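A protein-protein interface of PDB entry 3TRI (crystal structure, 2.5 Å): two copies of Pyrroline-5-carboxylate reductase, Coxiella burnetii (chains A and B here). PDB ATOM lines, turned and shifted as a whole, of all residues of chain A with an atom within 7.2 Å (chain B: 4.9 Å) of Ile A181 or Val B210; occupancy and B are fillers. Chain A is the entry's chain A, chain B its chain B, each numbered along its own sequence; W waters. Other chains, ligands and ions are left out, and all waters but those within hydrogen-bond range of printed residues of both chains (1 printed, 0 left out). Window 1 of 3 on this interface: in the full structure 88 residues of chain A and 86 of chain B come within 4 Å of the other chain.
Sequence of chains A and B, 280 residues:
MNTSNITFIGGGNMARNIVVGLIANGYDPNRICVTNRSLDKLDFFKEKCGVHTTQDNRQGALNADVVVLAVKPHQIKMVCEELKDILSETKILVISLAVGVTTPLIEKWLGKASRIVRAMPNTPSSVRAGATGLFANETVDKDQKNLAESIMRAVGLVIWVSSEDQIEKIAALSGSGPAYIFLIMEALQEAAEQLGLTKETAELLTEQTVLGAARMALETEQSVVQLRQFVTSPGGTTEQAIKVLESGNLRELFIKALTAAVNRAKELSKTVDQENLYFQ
Among the printed residues, merely in contact across the chains: Phe A182 with Ala B213, Leu A218 with Glu B207, Gly A177 with Thr B209, Ala A129 with Gly B212, Leu A218 with Leu B211, Ala A214 with Leu B211, Val A210 with Val B210, Pro A124 with Gly B212, Leu A211 with Ala B214, Ala A213 with Ile B181, Leu A211 with Leu B211, Pro A178 with Thr B209, Val A210 with Ala B214, Ile A181 with Ala B213, Ala A214 with Val B210, Val A210 with Ile B181, Ala A214 with Glu B207, Pro A124 with Ala B213, Glu A207 with Ala B214, Ile A181 with Val B210 and Phe A254 with Leu B188.
The side-chain amide nitrogen of Gln B208 lies within hydrogen-bond range of the backbone carbonyl oxygen of Ala A129 (3.1 Å).
Water W1 lies within hydrogen-bond range of O of Ala A129 (2.7 Å), O of Gln B208 (2.9 Å) and ND2 of Asn A122 (3.0 Å).
Of the 13 printed residues of chain B, 10 touch a printed residue of chain A.
Printed residues of chain B that touch a printed residue of chain A: Ile B181, Leu B188, Glu B207, Gln B208, Thr B209, Val B210, Leu B211, Gly B212, Ala B213 and Ala B214.
Hydrophobic or aromatic side chains of chain B within 4 Å of the printed part of chain A: Ile B181, Leu B188, Val B210, Leu B211, Ala B213 and Ala B214.
Hydrophobic or aromatic side chains of chain A within 4 Å of the printed part of chain B: Pro A124, Ala A129, Pro A178, Ile A181, Phe A182, Val A210, Leu A211, Ala A213, Ala A214, Leu A218 and Phe A254.
Among the printed residues, no Asp or Glu carboxylate lies within 4 Å of a Lys or Arg side-chain nitrogen of the other chain.
The backbone carbonyl oxygen of Pro A124 lies within hydrogen-bond range of the backbone NH of Ala A129, 3.0 Å away.
O of Leu B205 sits at hydrogen-bond distance from OG1 of Thr B209 (2.8 Å).
Glu A207 touches Ala B214, and with the chains exchanged Ala A214 touches Glu B207.
Val B210 touches its own counterpart, Val A210.
Leu A211 touches its own counterpart, Leu B211.
Leu A211 touches Ala B214, and with the chains exchanged Ala A214 touches Leu B211.
Of the 22 pairs that touch across the chains among the printed residues, 12 have their exchanged pair printed and touching as well.
Of the printed residues of chain B, Ile A181 touches Val B210 (3.9 Å) and Ala B213 (3.6 Å).
Of chain A, only Ile A181 (3.9 Å), Val A210 (3.4 Å) and Ala A214 (3.6 Å) come within 4 Å of Val B210.
Of the printed residues of chain B, Leu A218 touches Glu B207 (3.3 Å) and Leu B211 (3.4 Å).
Printed residues of chain A within 4 Å of Thr B209: Gly A177 (3.4 Å) and Pro A178 (3.5 Å).
Printed residues of chain A within 4 Å of Ile B181: Val A210 (3.6 Å) and Ala A213 (3.5 Å).
Of the printed residues of chain A, Leu B211 touches Leu A211, Ala A214 and Leu A218.
Printed residues of chain B within 4 Å of Pro A124: Gly B212 and Ala B213.
The nearest printed residue of chain B that does not touch Ile A181 is Thr B209 (4.02 Å).
The nearest printed residue of chain A that does not touch Gly B212 is Phe A182 (5.5 Å).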
ATOM      1  N   ASN A 122     -35.103 -15.203  14.403  1.00  0.00           N
ATOM      2  CA  ASN A 122     -33.721 -15.558  14.124  1.00  0.00           C
ATOM      3  C   ASN A 122     -33.126 -16.398  15.254  1.00  0.00           C
ATOM      4  O   ASN A 122     -33.707 -16.504  16.331  1.00  0.00           O
ATOM      5  CB  ASN A 122     -32.875 -14.315  13.818  1.00  0.00           C
ATOM      6  CG  ASN A 122     -32.792 -13.344  14.987  1.00  0.00           C
ATOM      7  OD1 ASN A 122     -33.179 -13.659  16.112  1.00  0.00           O
ATOM      8  ND2 ASN A 122     -32.270 -12.155  14.719  1.00  0.00           N
ATOM      9  N   PRO A 124     -30.680 -16.137  17.455  1.00  0.00           N
ATOM     10  CA  PRO A 124     -30.393 -15.604  18.793  1.00  0.00           C
ATOM     11  C   PRO A 124     -31.591 -15.673  19.740  1.00  0.00           C
ATOM     12  O   PRO A 124     -31.465 -15.300  20.909  1.00  0.00           O
ATOM     13  CB  PRO A 124     -30.013 -14.149  18.514  1.00  0.00           C
ATOM     14  CG  PRO A 124     -29.481 -14.171  17.129  1.00  0.00           C
ATOM     15  CD  PRO A 124     -30.320 -15.175  16.399  1.00  0.00           C
ATOM     16  N   ALA A 129     -32.341 -13.002  22.667  1.00  0.00           N
ATOM     17  CA  ALA A 129     -31.888 -11.739  22.105  1.00  0.00           C
ATOM     18  C   ALA A 129     -32.246 -11.736  20.639  1.00  0.00           C
ATOM     19  O   ALA A 129     -31.502 -11.224  19.802  1.00  0.00           O
ATOM     20  CB  ALA A 129     -30.389 -11.584  22.276  1.00  0.00           C
ATOM     21  N   SER A 176     -31.560 -13.534   8.218  1.00  0.00           N
ATOM     22  CA  SER A 176     -30.250 -14.013   7.793  1.00  0.00           C
ATOM     23  C   SER A 176     -29.140 -13.229   8.486  1.00  0.00           C
ATOM     24  O   SER A 176     -27.970 -13.611   8.441  1.00  0.00           O
ATOM     25  CB  SER A 176     -30.105 -13.869   6.275  1.00  0.00           C
ATOM     26  OG  SER A 176     -31.119 -14.578   5.587  1.00  0.00           O
ATOM     27  N   GLY A 177     -29.523 -12.126   9.122  1.00  0.00           N
ATOM     28  CA  GLY A 177     -28.580 -11.232   9.766  1.00  0.00           C
ATOM     29  C   GLY A 177     -27.516 -11.894  10.617  1.00  0.00           C
ATOM     30  O   GLY A 177     -26.331 -11.615  10.451  1.00  0.00           O
ATOM     31  N   PRO A 178     -27.928 -12.764  11.546  1.00  0.00           N
ATOM     32  CA  PRO A 178     -26.939 -13.363  12.448  1.00  0.00           C
ATOM     33  C   PRO A 178     -25.819 -14.073  11.686  1.00  0.00           C
ATOM     34  O   PRO A 178     -24.675 -14.063  12.141  1.00  0.00           O
ATOM     35  CB  PRO A 178     -27.771 -14.350  13.269  1.00  0.00           C
ATOM     36  CG  PRO A 178     -29.160 -13.751  13.259  1.00  0.00           C
ATOM     37  CD  PRO A 178     -29.306 -13.157  11.888  1.00  0.00           C
ATOM     38  N   ALA A 179     -26.134 -14.666  10.540  1.00  0.00           N
ATOM     39  CA  ALA A 179     -25.106 -15.318   9.735  1.00  0.00           C
ATOM     40  C   ALA A 179     -24.085 -14.304   9.227  1.00  0.00           C
ATOM     41  O   ALA A 179     -22.889 -14.592   9.188  1.00  0.00           O
ATOM     42  CB  ALA A 179     -25.720 -16.089   8.580  1.00  0.00           C
ATOM     43  N   TYR A 180     -24.556 -13.123   8.837  1.00  0.00           N
ATOM     44  CA  TYR A 180     -23.658 -12.065   8.380  1.00  0.00           C
ATOM     45  C   TYR A 180     -22.694 -11.707   9.497  1.00  0.00           C
ATOM     46  O   TYR A 180     -21.483 -11.620   9.292  1.00  0.00           O
ATOM     47  CB  TYR A 180     -24.435 -10.814   7.973  1.00  0.00           C
ATOM     48  CG  TYR A 180     -25.584 -11.070   7.028  1.00  0.00           C
ATOM     49  CD1 TYR A 180     -25.589 -12.176   6.187  1.00  0.00           C
ATOM     50  CD2 TYR A 180     -26.667 -10.203   6.978  1.00  0.00           C
ATOM     51  CE1 TYR A 180     -26.643 -12.410   5.324  1.00  0.00           C
ATOM     52  CE2 TYR A 180     -27.722 -10.424   6.121  1.00  0.00           C
ATOM     53  CZ  TYR A 180     -27.708 -11.528   5.297  1.00  0.00           C
ATOM     54  OH  TYR A 180     -28.763 -11.747   4.444  1.00  0.00           O
ATOM     55  N   ILE A 181     -23.247 -11.500  10.687  1.00  0.00           N
ATOM     56  CA  ILE A 181     -22.444 -11.154  11.847  1.00  0.00           C
ATOM     57  C   ILE A 181     -21.456 -12.269  12.174  1.00  0.00           C
ATOM     58  O   ILE A 181     -20.292 -12.006  12.472  1.00  0.00           O
ATOM     59  CB  ILE A 181     -23.324 -10.868  13.071  1.00  0.00           C
ATOM     60  CG1 ILE A 181     -24.432  -9.885  12.698  1.00  0.00           C
ATOM     61  CG2 ILE A 181     -22.481 -10.338  14.223  1.00  0.00           C
ATOM     62  CD1 ILE A 181     -23.954  -8.717  11.863  1.00  0.00           C
ATOM     63  N   PHE A 182     -21.923 -13.511  12.114  1.00  0.00           N
ATOM     64  CA  PHE A 182     -21.061 -14.654  12.387  1.00  0.00           C
ATOM     65  C   PHE A 182     -19.900 -14.693  11.403  1.00  0.00           C
ATOM     66  O   PHE A 182     -18.787 -15.084  11.756  1.00  0.00           O
ATOM     67  CB  PHE A 182     -21.855 -15.961  12.339  1.00  0.00           C
ATOM     68  CG  PHE A 182     -22.845 -16.101  13.457  1.00  0.00           C
ATOM     69  CD1 PHE A 182     -22.572 -15.572  14.702  1.00  0.00           C
ATOM     70  CD2 PHE A 182     -24.056 -16.738  13.257  1.00  0.00           C
ATOM     71  CE1 PHE A 182     -23.480 -15.680  15.736  1.00  0.00           C
ATOM     72  CE2 PHE A 182     -24.972 -16.850  14.290  1.00  0.00           C
ATOM     73  CZ  PHE A 182     -24.680 -16.321  15.529  1.00  0.00           C
ATOM     74  N   LEU A 183     -20.164 -14.272  10.169  1.00  0.00           N
ATOM     75  CA  LEU A 183     -19.138 -14.250   9.133  1.00  0.00           C
ATOM     76  C   LEU A 183     -18.126 -13.139   9.389  1.00  0.00           C
ATOM     77  O   LEU A 183     -16.924 -13.351   9.278  1.00  0.00           O
ATOM     78  CB  LEU A 183     -19.764 -14.072   7.751  1.00  0.00           C
ATOM     79  CG  LEU A 183     -18.794 -14.271   6.584  1.00  0.00           C
ATOM     80  CD1 LEU A 183     -18.507 -15.750   6.405  1.00  0.00           C
ATOM     81  CD2 LEU A 183     -19.352 -13.675   5.298  1.00  0.00           C
ATOM     82  N   ILE A 184     -18.620 -11.953   9.722  1.00  0.00           N
ATOM     83  CA  ILE A 184     -17.748 -10.843  10.074  1.00  0.00           C
ATOM     84  C   ILE A 184     -16.889 -11.204  11.281  1.00  0.00           C
ATOM     85  O   ILE A 184     -15.689 -10.938  11.301  1.00  0.00           O
ATOM     86  CB  ILE A 184     -18.542  -9.554  10.379  1.00  0.00           C
ATOM     87  CG1 ILE A 184     -18.800  -8.761   9.095  1.00  0.00           C
ATOM     88  CG2 ILE A 184     -17.778  -8.675  11.356  1.00  0.00           C
ATOM     89  CD1 ILE A 184     -19.784  -9.405   8.163  1.00  0.00           C
ATOM     90  N   MET A 185     -17.506 -11.814  12.287  1.00  0.00           N
ATOM     91  CA  MET A 185     -16.782 -12.198  13.489  1.00  0.00           C
ATOM     92  C   MET A 185     -15.682 -13.194  13.163  1.00  0.00           C
ATOM     93  O   MET A 185     -14.573 -13.101  13.682  1.00  0.00           O
ATOM     94  CB  MET A 185     -17.734 -12.781  14.531  1.00  0.00           C
ATOM     95  CG  MET A 185     -18.768 -11.783  15.018  1.00  0.00           C
ATOM     96  SD  MET A 185     -19.725 -12.386  16.604  1.00  0.00           S
ATOM     97  CE  MET A 185     -20.176 -14.181  16.017  1.00  0.00           C
ATOM     98  N   GLU A 186     -16.002 -14.144  12.294  1.00  0.00           N
ATOM     99  CA  GLU A 186     -15.031 -15.124  11.844  1.00  0.00           C
ATOM    100  C   GLU A 186     -13.869 -14.418  11.156  1.00  0.00           C
ATOM    101  O   GLU A 186     -12.704 -14.655  11.483  1.00  0.00           O
ATOM    102  CB  GLU A 186     -15.694 -16.113  10.886  1.00  0.00           C
ATOM    103  CG  GLU A 186     -14.814 -17.269  10.469  1.00  0.00           C
ATOM    104  CD  GLU A 186     -15.420 -18.065   9.333  1.00  0.00           C
ATOM    105  OE1 GLU A 186     -16.621 -17.870   9.054  1.00  0.00           O
ATOM    106  OE2 GLU A 186     -14.695 -18.874   8.716  1.00  0.00           O
ATOM    107  N   ALA A 187     -14.197 -13.539  10.214  1.00  0.00           N
ATOM    108  CA  ALA A 187     -13.193 -12.796   9.463  1.00  0.00           C
ATOM    109  C   ALA A 187     -12.362 -11.917  10.386  1.00  0.00           C
ATOM    110  O   ALA A 187     -11.152 -11.795  10.218  1.00  0.00           O
ATOM    111  CB  ALA A 187     -13.853 -11.952   8.386  1.00  0.00           C
ATOM    112  N   THR A 206     -13.308 -10.513  19.992  1.00  0.00           N
ATOM    113  CA  THR A 206     -14.186 -10.299  18.851  1.00  0.00           C
ATOM    114  C   THR A 206     -15.641 -10.359  19.300  1.00  0.00           C
ATOM    115  O   THR A 206     -16.412  -9.426  19.066  1.00  0.00           O
ATOM    116  CB  THR A 206     -13.944 -11.332  17.734  1.00  0.00           C
ATOM    117  OG1 THR A 206     -12.629 -11.157  17.194  1.00  0.00           O
ATOM    118  CG2 THR A 206     -14.961 -11.158  16.617  1.00  0.00           C
ATOM    119  N   GLU A 207     -16.005 -11.456  19.956  1.00  0.00           N
ATOM    120  CA  GLU A 207     -17.350 -11.622  20.491  1.00  0.00           C
ATOM    121  C   GLU A 207     -17.770 -10.422  21.330  1.00  0.00           C
ATOM    122  O   GLU A 207     -18.813  -9.813  21.081  1.00  0.00           O
ATOM    123  CB  GLU A 207     -17.437 -12.896  21.339  1.00  0.00           C
ATOM    124  CG  GLU A 207     -17.386 -14.191  20.538  1.00  0.00           C
ATOM    125  CD  GLU A 207     -17.372 -15.425  21.425  1.00  0.00           C
ATOM    126  OE1 GLU A 207     -17.263 -15.269  22.661  1.00  0.00           O
ATOM    127  OE2 GLU A 207     -17.470 -16.548  20.888  1.00  0.00           O
ATOM    128  N   THR A 209     -16.418  -7.475  21.607  1.00  0.00           N
ATOM    129  CA  THR A 209     -16.345  -6.219  20.880  1.00  0.00           C
ATOM    130  C   THR A 209     -17.631  -5.978  20.100  1.00  0.00           C
ATOM    131  O   THR A 209     -18.158  -4.864  20.069  1.00  0.00           O
ATOM    132  CB  THR A 209     -15.143  -6.213  19.926  1.00  0.00           C
ATOM    133  OG1 THR A 209     -13.935  -6.130  20.692  1.00  0.00           O
ATOM    134  CG2 THR A 209     -15.220  -5.033  18.972  1.00  0.00           C
ATOM    135  N   VAL A 210     -18.134  -7.033  19.471  1.00  0.00           N
ATOM    136  CA  VAL A 210     -19.371  -6.944  18.714  1.00  0.00           C
ATOM    137  C   VAL A 210     -20.544  -6.658  19.647  1.00  0.00           C
ATOM    138  O   VAL A 210     -21.371  -5.791  19.371  1.00  0.00           O
ATOM    139  CB  VAL A 210     -19.615  -8.231  17.901  1.00  0.00           C
ATOM    140  CG1 VAL A 210     -21.048  -8.299  17.400  1.00  0.00           C
ATOM    141  CG2 VAL A 210     -18.625  -8.309  16.741  1.00  0.00           C
ATOM    142  N   LEU A 211     -20.599  -7.382  20.760  1.00  0.00           N
ATOM    143  CA  LEU A 211     -21.632  -7.172  21.769  1.00  0.00           C
ATOM    144  C   LEU A 211     -21.636  -5.733  22.267  1.00  0.00           C
ATOM    145  O   LEU A 211     -22.687  -5.092  22.339  1.00  0.00           O
ATOM    146  CB  LEU A 211     -21.417  -8.110  22.955  1.00  0.00           C
ATOM    147  CG  LEU A 211     -22.428  -7.958  24.093  1.00  0.00           C
ATOM    148  CD1 LEU A 211     -23.728  -8.658  23.732  1.00  0.00           C
ATOM    149  CD2 LEU A 211     -21.866  -8.516  25.389  1.00  0.00           C
ATOM    150  N   GLY A 212     -20.454  -5.239  22.625  1.00  0.00           N
ATOM    151  CA  GLY A 212     -20.311  -3.902  23.164  1.00  0.00           C
ATOM    152  C   GLY A 212     -20.741  -2.835  22.180  1.00  0.00           C
ATOM    153  O   GLY A 212     -21.323  -1.822  22.567  1.00  0.00           O
ATOM    154  N   ALA A 213     -20.454  -3.063  20.902  1.00  0.00           N
ATOM    155  CA  ALA A 213     -20.834  -2.127  19.855  1.00  0.00           C
ATOM    156  C   ALA A 213     -22.352  -2.040  19.712  1.00  0.00           C
ATOM    157  O   ALA A 213     -22.907  -0.949  19.575  1.00  0.00           O
ATOM    158  CB  ALA A 213     -20.193  -2.522  18.534  1.00  0.00           C
ATOM    159  N   ALA A 214     -23.018  -3.192  19.741  1.00  0.00           N
ATOM    160  CA  ALA A 214     -24.475  -3.248  19.639  1.00  0.00           C
ATOM    161  C   ALA A 214     -25.122  -2.608  20.864  1.00  0.00           C
ATOM    162  O   ALA A 214     -26.110  -1.875  20.748  1.00  0.00           O
ATOM    163  CB  ALA A 214     -24.945  -4.685  19.476  1.00  0.00           C
ATOM    164  N   ARG A 215     -24.554  -2.885  22.034  1.00  0.00           N
ATOM    165  CA  ARG A 215     -25.035  -2.305  23.284  1.00  0.00           C
ATOM    166  C   ARG A 215     -24.990  -0.785  23.251  1.00  0.00           C
ATOM    167  O   ARG A 215     -25.973  -0.123  23.577  1.00  0.00           O
ATOM    168  CB  ARG A 215     -24.229  -2.831  24.473  1.00  0.00           C
ATOM    169  CG  ARG A 215     -24.789  -4.109  25.075  1.00  0.00           C
ATOM    170  CD  ARG A 215     -25.632  -3.822  26.307  1.00  0.00           C
ATOM    171  NE  ARG A 215     -24.811  -3.777  27.512  1.00  0.00           N
ATOM    172  CZ  ARG A 215     -24.411  -4.855  28.179  1.00  0.00           C
ATOM    173  NH1 ARG A 215     -24.763  -6.063  27.759  1.00  0.00           N
ATOM    174  NH2 ARG A 215     -23.661  -4.727  29.266  1.00  0.00           N
ATOM    175  N   LEU A 218     -27.682   0.375  21.039  1.00  0.00           N
ATOM    176  CA  LEU A 218     -29.024   0.203  21.585  1.00  0.00           C
ATOM    177  C   LEU A 218     -29.342   1.145  22.737  1.00  0.00           C
ATOM    178  O   LEU A 218     -30.504   1.469  22.974  1.00  0.00           O
ATOM    179  CB  LEU A 218     -29.229  -1.242  22.036  1.00  0.00           C
ATOM    180  CG  LEU A 218     -29.366  -2.264  20.908  1.00  0.00           C
ATOM    181  CD1 LEU A 218     -29.122  -3.664  21.438  1.00  0.00           C
ATOM    182  CD2 LEU A 218     -30.732  -2.154  20.241  1.00  0.00           C
ATOM    183  N   PHE A 254     -23.033  -5.222   1.080  1.00  0.00           N
ATOM    184  CA  PHE A 254     -24.224  -5.632   1.828  1.00  0.00           C
ATOM    185  C   PHE A 254     -25.518  -5.471   1.030  1.00  0.00           C
ATOM    186  O   PHE A 254     -26.402  -6.324   1.094  1.00  0.00           O
ATOM    187  CB  PHE A 254     -24.318  -4.892   3.168  1.00  0.00           C
ATOM    188  CG  PHE A 254     -23.642  -5.614   4.301  1.00  0.00           C
ATOM    189  CD1 PHE A 254     -24.266  -6.680   4.929  1.00  0.00           C
ATOM    190  CD2 PHE A 254     -22.381  -5.238   4.731  1.00  0.00           C
ATOM    191  CE1 PHE A 254     -23.646  -7.357   5.967  1.00  0.00           C
ATOM    192  CE2 PHE A 254     -21.755  -5.909   5.766  1.00  0.00           C
ATOM    193  CZ  PHE A 254     -22.387  -6.970   6.386  1.00  0.00           C
ATOM    194  N   ILE B 181     -17.559  -2.372  13.861  1.00  0.00           N
ATOM    195  CA  ILE B 181     -18.936  -2.845  13.936  1.00  0.00           C
ATOM    196  C   ILE B 181     -19.919  -1.730  13.595  1.00  0.00           C
ATOM    197  O   ILE B 181     -20.928  -1.964  12.930  1.00  0.00           O
ATOM    198  CB  ILE B 181     -19.263  -3.415  15.322  1.00  0.00           C
ATOM    199  CG1 ILE B 181     -18.161  -4.376  15.764  1.00  0.00           C
ATOM    200  CG2 ILE B 181     -20.616  -4.115  15.307  1.00  0.00           C
ATOM    201  CD1 ILE B 181     -17.803  -5.408  14.712  1.00  0.00           C
ATOM    202  N   MET B 185     -22.547  -2.125  10.820  1.00  0.00           N
ATOM    203  CA  MET B 185     -23.955  -1.881  11.095  1.00  0.00           C
ATOM    204  C   MET B 185     -24.542  -0.812  10.188  1.00  0.00           C
ATOM    205  O   MET B 185     -25.669  -0.944   9.717  1.00  0.00           O
ATOM    206  CB  MET B 185     -24.159  -1.509  12.554  1.00  0.00           C
ATOM    207  CG  MET B 185     -23.888  -2.654  13.498  1.00  0.00           C
ATOM    208  SD  MET B 185     -24.286  -2.151  15.326  1.00  0.00           S
ATOM    209  CE  MET B 185     -22.973  -0.749  15.527  1.00  0.00           C
ATOM    210  N   LEU B 188     -24.929  -2.383   6.741  1.00  0.00           N
ATOM    211  CA  LEU B 188     -26.029  -3.336   6.814  1.00  0.00           C
ATOM    212  C   LEU B 188     -27.369  -2.614   6.942  1.00  0.00           C
ATOM    213  O   LEU B 188     -28.333  -2.944   6.253  1.00  0.00           O
ATOM    214  CB  LEU B 188     -25.817  -4.292   7.988  1.00  0.00           C
ATOM    215  CG  LEU B 188     -26.948  -5.265   8.314  1.00  0.00           C
ATOM    216  CD1 LEU B 188     -27.518  -5.894   7.055  1.00  0.00           C
ATOM    217  CD2 LEU B 188     -26.457  -6.330   9.278  1.00  0.00           C
ATOM    218  N   LEU B 205     -33.514  -3.422  13.955  1.00  0.00           N
ATOM    219  CA  LEU B 205     -33.237  -4.806  13.602  1.00  0.00           C
ATOM    220  C   LEU B 205     -31.743  -5.069  13.469  1.00  0.00           C
ATOM    221  O   LEU B 205     -31.245  -6.098  13.922  1.00  0.00           O
ATOM    222  CB  LEU B 205     -33.965  -5.190  12.315  1.00  0.00           C
ATOM    223  CG  LEU B 205     -35.486  -5.288  12.442  1.00  0.00           C
ATOM    224  CD1 LEU B 205     -36.113  -5.582  11.091  1.00  0.00           C
ATOM    225  CD2 LEU B 205     -35.863  -6.351  13.463  1.00  0.00           C
ATOM    226  N   THR B 206     -31.032  -4.138  12.843  1.00  0.00           N
ATOM    227  CA  THR B 206     -29.593  -4.280  12.673  1.00  0.00           C
ATOM    228  C   THR B 206     -28.900  -4.411  14.019  1.00  0.00           C
ATOM    229  O   THR B 206     -28.057  -5.286  14.212  1.00  0.00           O
ATOM    230  CB  THR B 206     -28.993  -3.090  11.915  1.00  0.00           C
ATOM    231  OG1 THR B 206     -29.430  -3.131  10.554  1.00  0.00           O
ATOM    232  CG2 THR B 206     -27.477  -3.154  11.946  1.00  0.00           C
ATOM    233  N   GLU B 207     -29.271  -3.543  14.953  1.00  0.00           N
ATOM    234  CA  GLU B 207     -28.663  -3.542  16.275  1.00  0.00           C
ATOM    235  C   GLU B 207     -29.017  -4.795  17.066  1.00  0.00           C
ATOM    236  O   GLU B 207     -28.153  -5.410  17.685  1.00  0.00           O
ATOM    237  CB  GLU B 207     -29.081  -2.287  17.038  1.00  0.00           C
ATOM    238  CG  GLU B 207     -28.657  -1.009  16.343  1.00  0.00           C
ATOM    239  CD  GLU B 207     -29.310   0.216  16.935  1.00  0.00           C
ATOM    240  OE1 GLU B 207     -30.169   0.049  17.828  1.00  0.00           O
ATOM    241  OE2 GLU B 207     -28.966   1.339  16.504  1.00  0.00           O
ATOM    242  N   GLN B 208     -30.291  -5.172  17.047  1.00  0.00           N
ATOM    243  CA  GLN B 208     -30.720  -6.378  17.737  1.00  0.00           C
ATOM    244  C   GLN B 208     -30.035  -7.590  17.135  1.00  0.00           C
ATOM    245  O   GLN B 208     -29.632  -8.507  17.853  1.00  0.00           O
ATOM    246  CB  GLN B 208     -32.235  -6.549  17.642  1.00  0.00           C
ATOM    247  CG  GLN B 208     -32.769  -7.715  18.455  1.00  0.00           C
ATOM    248  CD  GLN B 208     -32.555  -7.541  19.951  1.00  0.00           C
ATOM    249  OE1 GLN B 208     -32.134  -6.481  20.415  1.00  0.00           O
ATOM    250  NE2 GLN B 208     -32.854  -8.587  20.712  1.00  0.00           N
ATOM    251  N   THR B 209     -29.911  -7.592  15.811  1.00  0.00           N
ATOM    252  CA  THR B 209     -29.260  -8.693  15.113  1.00  0.00           C
ATOM    253  C   THR B 209     -27.817  -8.827  15.582  1.00  0.00           C
ATOM    254  O   THR B 209     -27.361  -9.923  15.909  1.00  0.00           O
ATOM    255  CB  THR B 209     -29.310  -8.520  13.578  1.00  0.00           C
ATOM    256  OG1 THR B 209     -30.660  -8.684  13.121  1.00  0.00           O
ATOM    257  CG2 THR B 209     -28.432  -9.554  12.892  1.00  0.00           C
ATOM    258  N   VAL B 210     -27.110  -7.702  15.627  1.00  0.00           N
ATOM    259  CA  VAL B 210     -25.727  -7.692  16.084  1.00  0.00           C
ATOM    260  C   VAL B 210     -25.649  -8.136  17.543  1.00  0.00           C
ATOM    261  O   VAL B 210     -24.859  -9.009  17.892  1.00  0.00           O
ATOM    262  CB  VAL B 210     -25.078  -6.303  15.901  1.00  0.00           C
ATOM    263  CG1 VAL B 210     -23.677  -6.291  16.480  1.00  0.00           C
ATOM    264  CG2 VAL B 210     -25.046  -5.928  14.425  1.00  0.00           C
ATOM    265  N   LEU B 211     -26.482  -7.541  18.388  1.00  0.00           N
ATOM    266  CA  LEU B 211     -26.549  -7.930  19.791  1.00  0.00           C
ATOM    267  C   LEU B 211     -26.757  -9.434  19.938  1.00  0.00           C
ATOM    268  O   LEU B 211     -26.026 -10.103  20.667  1.00  0.00           O
ATOM    269  CB  LEU B 211     -27.682  -7.186  20.501  1.00  0.00           C
ATOM    270  CG  LEU B 211     -27.807  -7.462  22.000  1.00  0.00           C
ATOM    271  CD1 LEU B 211     -26.603  -6.907  22.744  1.00  0.00           C
ATOM    272  CD2 LEU B 211     -29.090  -6.876  22.555  1.00  0.00           C
ATOM    273  N   GLY B 212     -27.760  -9.955  19.237  1.00  0.00           N
ATOM    274  CA  GLY B 212     -28.142 -11.349  19.357  1.00  0.00           C
ATOM    275  C   GLY B 212     -27.074 -12.327  18.912  1.00  0.00           C
ATOM    276  O   GLY B 212     -26.840 -13.341  19.570  1.00  0.00           O
ATOM    277  N   ALA B 213     -26.429 -12.031  17.788  1.00  0.00           N
ATOM    278  CA  ALA B 213     -25.361 -12.883  17.280  1.00  0.00           C
ATOM    279  C   ALA B 213     -24.182 -12.909  18.253  1.00  0.00           C
ATOM    280  O   ALA B 213     -23.563 -13.949  18.467  1.00  0.00           O
ATOM    281  CB  ALA B 213     -24.915 -12.414  15.902  1.00  0.00           C
ATOM    282  N   ALA B 214     -23.889 -11.757  18.849  1.00  0.00           N
ATOM    283  CA  ALA B 214     -22.799 -11.644  19.808  1.00  0.00           C
ATOM    284  C   ALA B 214     -23.130 -12.388  21.100  1.00  0.00           C
ATOM    285  O   ALA B 214     -22.297 -13.118  21.630  1.00  0.00           O
ATOM    286  CB  ALA B 214     -22.485 -10.181  20.089  1.00  0.00           C
HETATM  287  O   HOH W   1     -31.115 -10.957  17.170  1.00  0.00           O
